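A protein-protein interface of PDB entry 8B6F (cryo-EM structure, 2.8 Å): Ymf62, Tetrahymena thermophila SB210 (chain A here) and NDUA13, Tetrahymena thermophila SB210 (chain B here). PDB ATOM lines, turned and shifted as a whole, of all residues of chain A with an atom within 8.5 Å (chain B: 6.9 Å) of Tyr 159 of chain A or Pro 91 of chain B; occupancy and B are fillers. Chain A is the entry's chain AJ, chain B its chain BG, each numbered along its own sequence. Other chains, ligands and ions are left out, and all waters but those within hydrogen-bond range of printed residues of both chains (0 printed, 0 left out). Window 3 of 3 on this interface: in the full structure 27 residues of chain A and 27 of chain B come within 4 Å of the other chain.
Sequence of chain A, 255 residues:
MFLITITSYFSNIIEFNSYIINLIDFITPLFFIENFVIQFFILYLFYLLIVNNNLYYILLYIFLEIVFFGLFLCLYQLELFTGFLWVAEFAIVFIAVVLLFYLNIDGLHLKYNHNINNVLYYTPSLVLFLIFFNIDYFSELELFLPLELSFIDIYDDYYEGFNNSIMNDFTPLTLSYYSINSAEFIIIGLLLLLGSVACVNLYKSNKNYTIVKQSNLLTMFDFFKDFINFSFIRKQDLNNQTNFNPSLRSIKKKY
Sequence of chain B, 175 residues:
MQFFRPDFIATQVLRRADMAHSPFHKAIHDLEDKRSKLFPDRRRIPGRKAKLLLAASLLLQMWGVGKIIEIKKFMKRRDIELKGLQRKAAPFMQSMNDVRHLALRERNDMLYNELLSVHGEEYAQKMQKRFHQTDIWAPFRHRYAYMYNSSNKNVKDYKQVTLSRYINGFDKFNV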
ATOM      1  N   TYR A 155       3.415  38.632  -5.008  1.00  0.00           N
ATOM      2  CA  TYR A 155       2.509  38.081  -4.010  1.00  0.00           C
ATOM      3  C   TYR A 155       2.337  36.580  -4.204  1.00  0.00           C
ATOM      4  O   TYR A 155       2.178  36.095  -5.326  1.00  0.00           O
ATOM      5  CB  TYR A 155       1.151  38.780  -4.091  1.00  0.00           C
ATOM      6  CG  TYR A 155       0.127  38.232  -3.126  1.00  0.00           C
ATOM      7  CD1 TYR A 155       0.040  38.714  -1.827  1.00  0.00           C
ATOM      8  CD2 TYR A 155      -0.764  37.243  -3.518  1.00  0.00           C
ATOM      9  CE1 TYR A 155      -0.895  38.217  -0.943  1.00  0.00           C
ATOM     10  CE2 TYR A 155      -1.703  36.739  -2.642  1.00  0.00           C
ATOM     11  CZ  TYR A 155      -1.765  37.231  -1.357  1.00  0.00           C
ATOM     12  OH  TYR A 155      -2.701  36.732  -0.481  1.00  0.00           O
ATOM     13  N   ASP A 156       2.363  35.845  -3.094  1.00  0.00           N
ATOM     14  CA  ASP A 156       2.184  34.400  -3.095  1.00  0.00           C
ATOM     15  C   ASP A 156       1.148  34.020  -2.050  1.00  0.00           C
ATOM     16  O   ASP A 156       1.139  34.565  -0.943  1.00  0.00           O
ATOM     17  CB  ASP A 156       3.500  33.670  -2.809  1.00  0.00           C
ATOM     18  CG  ASP A 156       4.560  33.946  -3.856  1.00  0.00           C
ATOM     19  OD1 ASP A 156       4.194  34.169  -5.027  1.00  0.00           O
ATOM     20  OD2 ASP A 156       5.759  33.939  -3.507  1.00  0.00           O
ATOM     21  N   ASP A 157       0.282  33.077  -2.404  1.00  0.00           N
ATOM     22  CA  ASP A 157      -0.781  32.595  -1.527  1.00  0.00           C
ATOM     23  C   ASP A 157      -0.421  31.179  -1.092  1.00  0.00           C
ATOM     24  O   ASP A 157      -0.702  30.211  -1.803  1.00  0.00           O
ATOM     25  CB  ASP A 157      -2.129  32.639  -2.239  1.00  0.00           C
ATOM     26  CG  ASP A 157      -3.286  32.337  -1.314  1.00  0.00           C
ATOM     27  OD1 ASP A 157      -3.043  32.109  -0.111  1.00  0.00           O
ATOM     28  OD2 ASP A 157      -4.440  32.326  -1.787  1.00  0.00           O
ATOM     29  N   TYR A 158       0.213  31.064   0.078  1.00  0.00           N
ATOM     30  CA  TYR A 158       0.705  29.765   0.523  1.00  0.00           C
ATOM     31  C   TYR A 158      -0.424  28.860   0.997  1.00  0.00           C
ATOM     32  O   TYR A 158      -0.339  27.638   0.837  1.00  0.00           O
ATOM     33  CB  TYR A 158       1.744  29.951   1.628  1.00  0.00           C
ATOM     34  CG  TYR A 158       2.989  30.645   1.141  1.00  0.00           C
ATOM     35  CD1 TYR A 158       3.077  32.028   1.132  1.00  0.00           C
ATOM     36  CD2 TYR A 158       4.073  29.915   0.672  1.00  0.00           C
ATOM     37  CE1 TYR A 158       4.210  32.666   0.680  1.00  0.00           C
ATOM     38  CE2 TYR A 158       5.211  30.543   0.217  1.00  0.00           C
ATOM     39  CZ  TYR A 158       5.273  31.920   0.223  1.00  0.00           C
ATOM     40  OH  TYR A 158       6.404  32.551  -0.230  1.00  0.00           O
ATOM     41  N   TYR A 159      -1.481  29.428   1.577  1.00  0.00           N
ATOM     42  CA  TYR A 159      -2.620  28.609   1.978  1.00  0.00           C
ATOM     43  C   TYR A 159      -3.261  27.945   0.768  1.00  0.00           C
ATOM     44  O   TYR A 159      -3.513  26.735   0.768  1.00  0.00           O
ATOM     45  CB  TYR A 159      -3.636  29.452   2.745  1.00  0.00           C
ATOM     46  CG  TYR A 159      -3.293  29.606   4.207  1.00  0.00           C
ATOM     47  CD1 TYR A 159      -2.465  30.630   4.644  1.00  0.00           C
ATOM     48  CD2 TYR A 159      -3.785  28.713   5.148  1.00  0.00           C
ATOM     49  CE1 TYR A 159      -2.147  30.766   5.983  1.00  0.00           C
ATOM     50  CE2 TYR A 159      -3.475  28.840   6.485  1.00  0.00           C
ATOM     51  CZ  TYR A 159      -2.655  29.867   6.896  1.00  0.00           C
ATOM     52  OH  TYR A 159      -2.347  29.992   8.228  1.00  0.00           O
ATOM     53  N   GLU A 160      -3.544  28.726  -0.272  1.00  0.00           N
ATOM     54  CA  GLU A 160      -4.055  28.148  -1.508  1.00  0.00           C
ATOM     55  C   GLU A 160      -3.037  27.207  -2.135  1.00  0.00           C
ATOM     56  O   GLU A 160      -3.415  26.212  -2.762  1.00  0.00           O
ATOM     57  CB  GLU A 160      -4.438  29.257  -2.489  1.00  0.00           C
ATOM     58  CG  GLU A 160      -5.252  28.783  -3.688  1.00  0.00           C
ATOM     59  CD  GLU A 160      -4.404  28.153  -4.778  1.00  0.00           C
ATOM     60  OE1 GLU A 160      -3.168  28.333  -4.754  1.00  0.00           O
ATOM     61  OE2 GLU A 160      -4.974  27.483  -5.663  1.00  0.00           O
ATOM     62  N   GLY A 161      -1.747  27.504  -1.980  1.00  0.00           N
ATOM     63  CA  GLY A 161      -0.728  26.631  -2.539  1.00  0.00           C
ATOM     64  C   GLY A 161      -0.755  25.237  -1.943  1.00  0.00           C
ATOM     65  O   GLY A 161      -0.708  24.240  -2.666  1.00  0.00           O
ATOM     66  N   PHE A 162      -0.836  25.146  -0.616  1.00  0.00           N
ATOM     67  CA  PHE A 162      -0.874  23.837   0.022  1.00  0.00           C
ATOM     68  C   PHE A 162      -2.239  23.173  -0.089  1.00  0.00           C
ATOM     69  O   PHE A 162      -2.329  21.950   0.062  1.00  0.00           O
ATOM     70  CB  PHE A 162      -0.446  23.951   1.492  1.00  0.00           C
ATOM     71  CG  PHE A 162      -1.588  24.063   2.462  1.00  0.00           C
ATOM     72  CD1 PHE A 162      -2.246  22.937   2.927  1.00  0.00           C
ATOM     73  CD2 PHE A 162      -1.962  25.298   2.954  1.00  0.00           C
ATOM     74  CE1 PHE A 162      -3.283  23.049   3.832  1.00  0.00           C
ATOM     75  CE2 PHE A 162      -2.997  25.420   3.859  1.00  0.00           C
ATOM     76  CZ  PHE A 162      -3.659  24.293   4.300  1.00  0.00           C
ATOM     77  N   ASN A 163      -3.296  23.940  -0.352  1.00  0.00           N
ATOM     78  CA  ASN A 163      -4.594  23.353  -0.651  1.00  0.00           C
ATOM     79  C   ASN A 163      -4.726  22.926  -2.105  1.00  0.00           C
ATOM     80  O   ASN A 163      -5.690  22.231  -2.443  1.00  0.00           O
ATOM     81  CB  ASN A 163      -5.713  24.345  -0.320  1.00  0.00           C
ATOM     82  CG  ASN A 163      -5.926  24.510   1.170  1.00  0.00           C
ATOM     83  OD1 ASN A 163      -5.855  25.620   1.698  1.00  0.00           O
ATOM     84  ND2 ASN A 163      -6.187  23.406   1.858  1.00  0.00           N
ATOM     85  N   ASN A 164      -3.793  23.319  -2.967  1.00  0.00           N
ATOM     86  CA  ASN A 164      -3.854  22.986  -4.382  1.00  0.00           C
ATOM     87  C   ASN A 164      -3.118  21.677  -4.634  1.00  0.00           C
ATOM     88  O   ASN A 164      -1.955  21.527  -4.247  1.00  0.00           O
ATOM     89  CB  ASN A 164      -3.241  24.111  -5.217  1.00  0.00           C
ATOM     90  CG  ASN A 164      -3.515  23.957  -6.697  1.00  0.00           C
ATOM     91  OD1 ASN A 164      -3.708  22.848  -7.192  1.00  0.00           O
ATOM     92  ND2 ASN A 164      -3.534  25.073  -7.414  1.00  0.00           N
ATOM     93  N   GLN B  86       3.062  21.093   5.038  1.00  0.00           N
ATOM     94  CA  GLN B  86       2.962  22.367   4.335  1.00  0.00           C
ATOM     95  C   GLN B  86       2.017  23.318   5.057  1.00  0.00           C
ATOM     96  O   GLN B  86       2.270  24.526   5.126  1.00  0.00           O
ATOM     97  CB  GLN B  86       2.505  22.135   2.895  1.00  0.00           C
ATOM     98  CG  GLN B  86       3.533  21.408   2.042  1.00  0.00           C
ATOM     99  CD  GLN B  86       3.006  21.057   0.669  1.00  0.00           C
ATOM    100  OE1 GLN B  86       1.798  21.026   0.445  1.00  0.00           O
ATOM    101  NE2 GLN B  86       3.914  20.798  -0.263  1.00  0.00           N
ATOM    102  N   ARG B  87       0.921  22.790   5.602  1.00  0.00           N
ATOM    103  CA  ARG B  87       0.014  23.613   6.395  1.00  0.00           C
ATOM    104  C   ARG B  87       0.711  24.160   7.635  1.00  0.00           C
ATOM    105  O   ARG B  87       0.536  25.332   7.984  1.00  0.00           O
ATOM    106  CB  ARG B  87      -1.219  22.799   6.790  1.00  0.00           C
ATOM    107  CG  ARG B  87      -2.200  23.537   7.693  1.00  0.00           C
ATOM    108  CD  ARG B  87      -1.955  23.240   9.168  1.00  0.00           C
ATOM    109  NE  ARG B  87      -2.922  23.918  10.023  1.00  0.00           N
ATOM    110  CZ  ARG B  87      -2.822  25.180  10.420  1.00  0.00           C
ATOM    111  NH1 ARG B  87      -1.809  25.943  10.049  1.00  0.00           N
ATOM    112  NH2 ARG B  87      -3.763  25.687  11.211  1.00  0.00           N
ATOM    113  N   LYS B  88       1.499  23.327   8.316  1.00  0.00           N
ATOM    114  CA  LYS B  88       2.241  23.805   9.478  1.00  0.00           C
ATOM    115  C   LYS B  88       3.161  24.961   9.106  1.00  0.00           C
ATOM    116  O   LYS B  88       3.278  25.938   9.854  1.00  0.00           O
ATOM    117  CB  LYS B  88       3.049  22.659  10.086  1.00  0.00           C
ATOM    118  CG  LYS B  88       2.257  21.745  11.008  1.00  0.00           C
ATOM    119  CD  LYS B  88       3.181  20.798  11.757  1.00  0.00           C
ATOM    120  CE  LYS B  88       2.417  19.949  12.757  1.00  0.00           C
ATOM    121  NZ  LYS B  88       3.318  19.027  13.503  1.00  0.00           N
ATOM    122  N   ALA B  89       3.829  24.866   7.959  1.00  0.00           N
ATOM    123  CA  ALA B  89       4.767  25.897   7.534  1.00  0.00           C
ATOM    124  C   ALA B  89       4.090  27.101   6.894  1.00  0.00           C
ATOM    125  O   ALA B  89       4.737  28.142   6.737  1.00  0.00           O
ATOM    126  CB  ALA B  89       5.777  25.302   6.550  1.00  0.00           C
ATOM    127  N   ALA B  90       2.815  26.991   6.524  1.00  0.00           N
ATOM    128  CA  ALA B  90       2.178  28.038   5.727  1.00  0.00           C
ATOM    129  C   ALA B  90       2.096  29.377   6.445  1.00  0.00           C
ATOM    130  O   ALA B  90       2.491  30.393   5.848  1.00  0.00           O
ATOM    131  CB  ALA B  90       0.786  27.571   5.292  1.00  0.00           C
ATOM    132  N   PRO B  91       1.601  29.469   7.684  1.00  0.00           N
ATOM    133  CA  PRO B  91       1.272  30.799   8.228  1.00  0.00           C
ATOM    134  C   PRO B  91       2.446  31.764   8.259  1.00  0.00           C
ATOM    135  O   PRO B  91       2.256  32.963   8.028  1.00  0.00           O
ATOM    136  CB  PRO B  91       0.750  30.485   9.640  1.00  0.00           C
ATOM    137  CG  PRO B  91       1.245  29.124   9.951  1.00  0.00           C
ATOM    138  CD  PRO B  91       1.311  28.396   8.652  1.00  0.00           C
ATOM    139  N   PHE B  92       3.655  31.281   8.544  1.00  0.00           N
ATOM    140  CA  PHE B  92       4.790  32.187   8.690  1.00  0.00           C
ATOM    141  C   PHE B  92       5.203  32.776   7.347  1.00  0.00           C
ATOM    142  O   PHE B  92       5.441  33.984   7.235  1.00  0.00           O
ATOM    143  CB  PHE B  92       5.957  31.454   9.342  1.00  0.00           C
ATOM    144  CG  PHE B  92       5.603  30.820  10.649  1.00  0.00           C
ATOM    145  CD1 PHE B  92       5.635  31.561  11.812  1.00  0.00           C
ATOM    146  CD2 PHE B  92       5.221  29.494  10.714  1.00  0.00           C
ATOM    147  CE1 PHE B  92       5.307  30.993  13.016  1.00  0.00           C
ATOM    148  CE2 PHE B  92       4.889  28.916  11.920  1.00  0.00           C
ATOM    149  CZ  PHE B  92       4.930  29.669  13.074  1.00  0.00           C
ATOM    150  N   MET B  93       5.294  31.939   6.315  1.00  0.00           N
ATOM    151  CA  MET B  93       5.628  32.448   4.990  1.00  0.00           C
ATOM    152  C   MET B  93       4.554  33.400   4.487  1.00  0.00           C
ATOM    153  O   MET B  93       4.859  34.410   3.843  1.00  0.00           O
ATOM    154  CB  MET B  93       5.828  31.290   4.016  1.00  0.00           C
ATOM    155  CG  MET B  93       6.866  30.290   4.485  1.00  0.00           C
ATOM    156  SD  MET B  93       7.276  29.077   3.224  1.00  0.00           S
ATOM    157  CE  MET B  93       8.198  30.082   2.067  1.00  0.00           C
ATOM    158  N   GLN B  94       3.289  33.086   4.759  1.00  0.00           N
ATOM    159  CA  GLN B  94       2.208  33.989   4.385  1.00  0.00           C
ATOM    160  C   GLN B  94       2.354  35.334   5.084  1.00  0.00           C
ATOM    161  O   GLN B  94       2.147  36.387   4.471  1.00  0.00           O
ATOM    162  CB  GLN B  94       0.859  33.352   4.720  1.00  0.00           C
ATOM    163  CG  GLN B  94      -0.343  34.115   4.192  1.00  0.00           C
ATOM    164  CD  GLN B  94      -0.416  34.106   2.679  1.00  0.00           C
ATOM    165  OE1 GLN B  94       0.367  33.435   2.013  1.00  0.00           O
ATOM    166  NE2 GLN B  94      -1.364  34.852   2.128  1.00  0.00           N
ATOM    167  N   SER B  95       2.709  35.322   6.371  1.00  0.00           N
ATOM    168  CA  SER B  95       2.884  36.576   7.096  1.00  0.00           C
ATOM    169  C   SER B  95       4.016  37.400   6.500  1.00  0.00           C
ATOM    170  O   SER B  95       3.882  38.612   6.307  1.00  0.00           O
ATOM    171  CB  SER B  95       3.152  36.288   8.573  1.00  0.00           C
ATOM    172  OG  SER B  95       2.090  35.550   9.151  1.00  0.00           O
ATOM    173  N   MET B  96       5.149  36.758   6.204  1.00  0.00           N
ATOM    174  CA  MET B  96       6.266  37.484   5.612  1.00  0.00           C
ATOM    175  C   MET B  96       5.877  38.069   4.263  1.00  0.00           C
ATOM    176  O   MET B  96       6.174  39.231   3.970  1.00  0.00           O
ATOM    177  CB  MET B  96       7.475  36.563   5.461  1.00  0.00           C
ATOM    178  CG  MET B  96       7.945  35.943   6.761  1.00  0.00           C
ATOM    179  SD  MET B  96       9.228  34.707   6.512  1.00  0.00           S
ATOM    180  CE  MET B  96       9.072  33.771   8.029  1.00  0.00           C
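The backbone NH of Tyr 158 of chain A sits at hydrogen-bond distance from the side-chain amide oxygen of Gln 94 of chain B (3.1 Å).
The side-chain amide nitrogen of Gln 94 of chain B sits at hydrogen-bond distance from the side-chain hydroxyl of Tyr 155 of chain A (3.5 Å).
The side-chain amide oxygen of Gln 94 of chain B sits close to the backbone carbonyl oxygen of Asp 156 of chain A (3.3 Å).
The side-chain amide oxygen (OD1) of Asn 163 of chain A lies close to the backbone carbonyl oxygen (O) of Tyr 159 of chain A (2.8 Å).
The side-chain hydroxyl (OG) of Ser 95 of chain B sits at hydrogen-bond distance from the backbone carbonyl oxygen (O) of Pro 91 of chain B.
N of Glu 160 of chain A sits at hydrogen-bond distance from OD1 of Asp 157 of chain A.
Among the printed residues, pairs that only touch across the chains: Tyr 159 of chain A with Pro 91 of chain B (3.4 Å), Tyr 158 of chain A with Met 93 of chain B (3.5 Å), Phe 162 of chain A with Arg 87 of chain B (3.6 Å), Phe 162 of chain A with Gln 86 of chain B (3.7 Å) and Asp 157 of chain A with Gln 94 of chain B (3.8 Å).
Printed residues of chain B within 4 Å of Asp 156 of chain A: Gln 94 (3.3 Å).
Of the printed residues of chain B, Asp 157 of chain A touches Gln 94 (3.8 Å).
Of the printed residues of chain B, Tyr 158 of chain A touches Met 93 and Gln 94.
Tyr 159 of chain A touches just one residue of chain B: Pro 91.
Ala 90 of chain B touches none of the printed residues of chain A.
Pro 91 of chain B touches just one residue of chain A: Tyr 159 (3.4 Å).
Printed residues of chain A within 4 Å of Met 93 of chain B: Tyr 158 (3.5 Å).
Printed residues of chain A within 4 Å of Gln 94 of chain B: Tyr 155, Asp 156, Asp 157 and Tyr 158.
The nearest residue of chain B that does not touch Tyr 159 of chain A is Gln 94 of chain B (4.1 Å).
The nearest printed residue of chain A that does not touch Gln 94 of chain B is Tyr 159 of chain A (4.1 Å).
Printed residues of chain B that touch a printed residue of chain A: Gln 86, Arg 87, Pro 91, Met 93 and Gln 94.
Along chain B the printed residues that touch a printed residue of chain A span positions 86 to 94.
Of the 10 printed residues of chain A, 6 touch a printed residue of chain B.
Printed residues of chain A that touch a printed residue of chain B: Tyr 155, Asp 156, Asp 157, Tyr 158, Tyr 159 and Phe 162.
Hydrophobic or aromatic side chains of chain A that line the printed part of chain B: Tyr 155, Tyr 158, Tyr 159 and Phe 162.
Along chain A the printed residues that touch a printed residue of chain B span positions 155 to 162.
Among the printed residues, 8 pairs touch across the chains.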
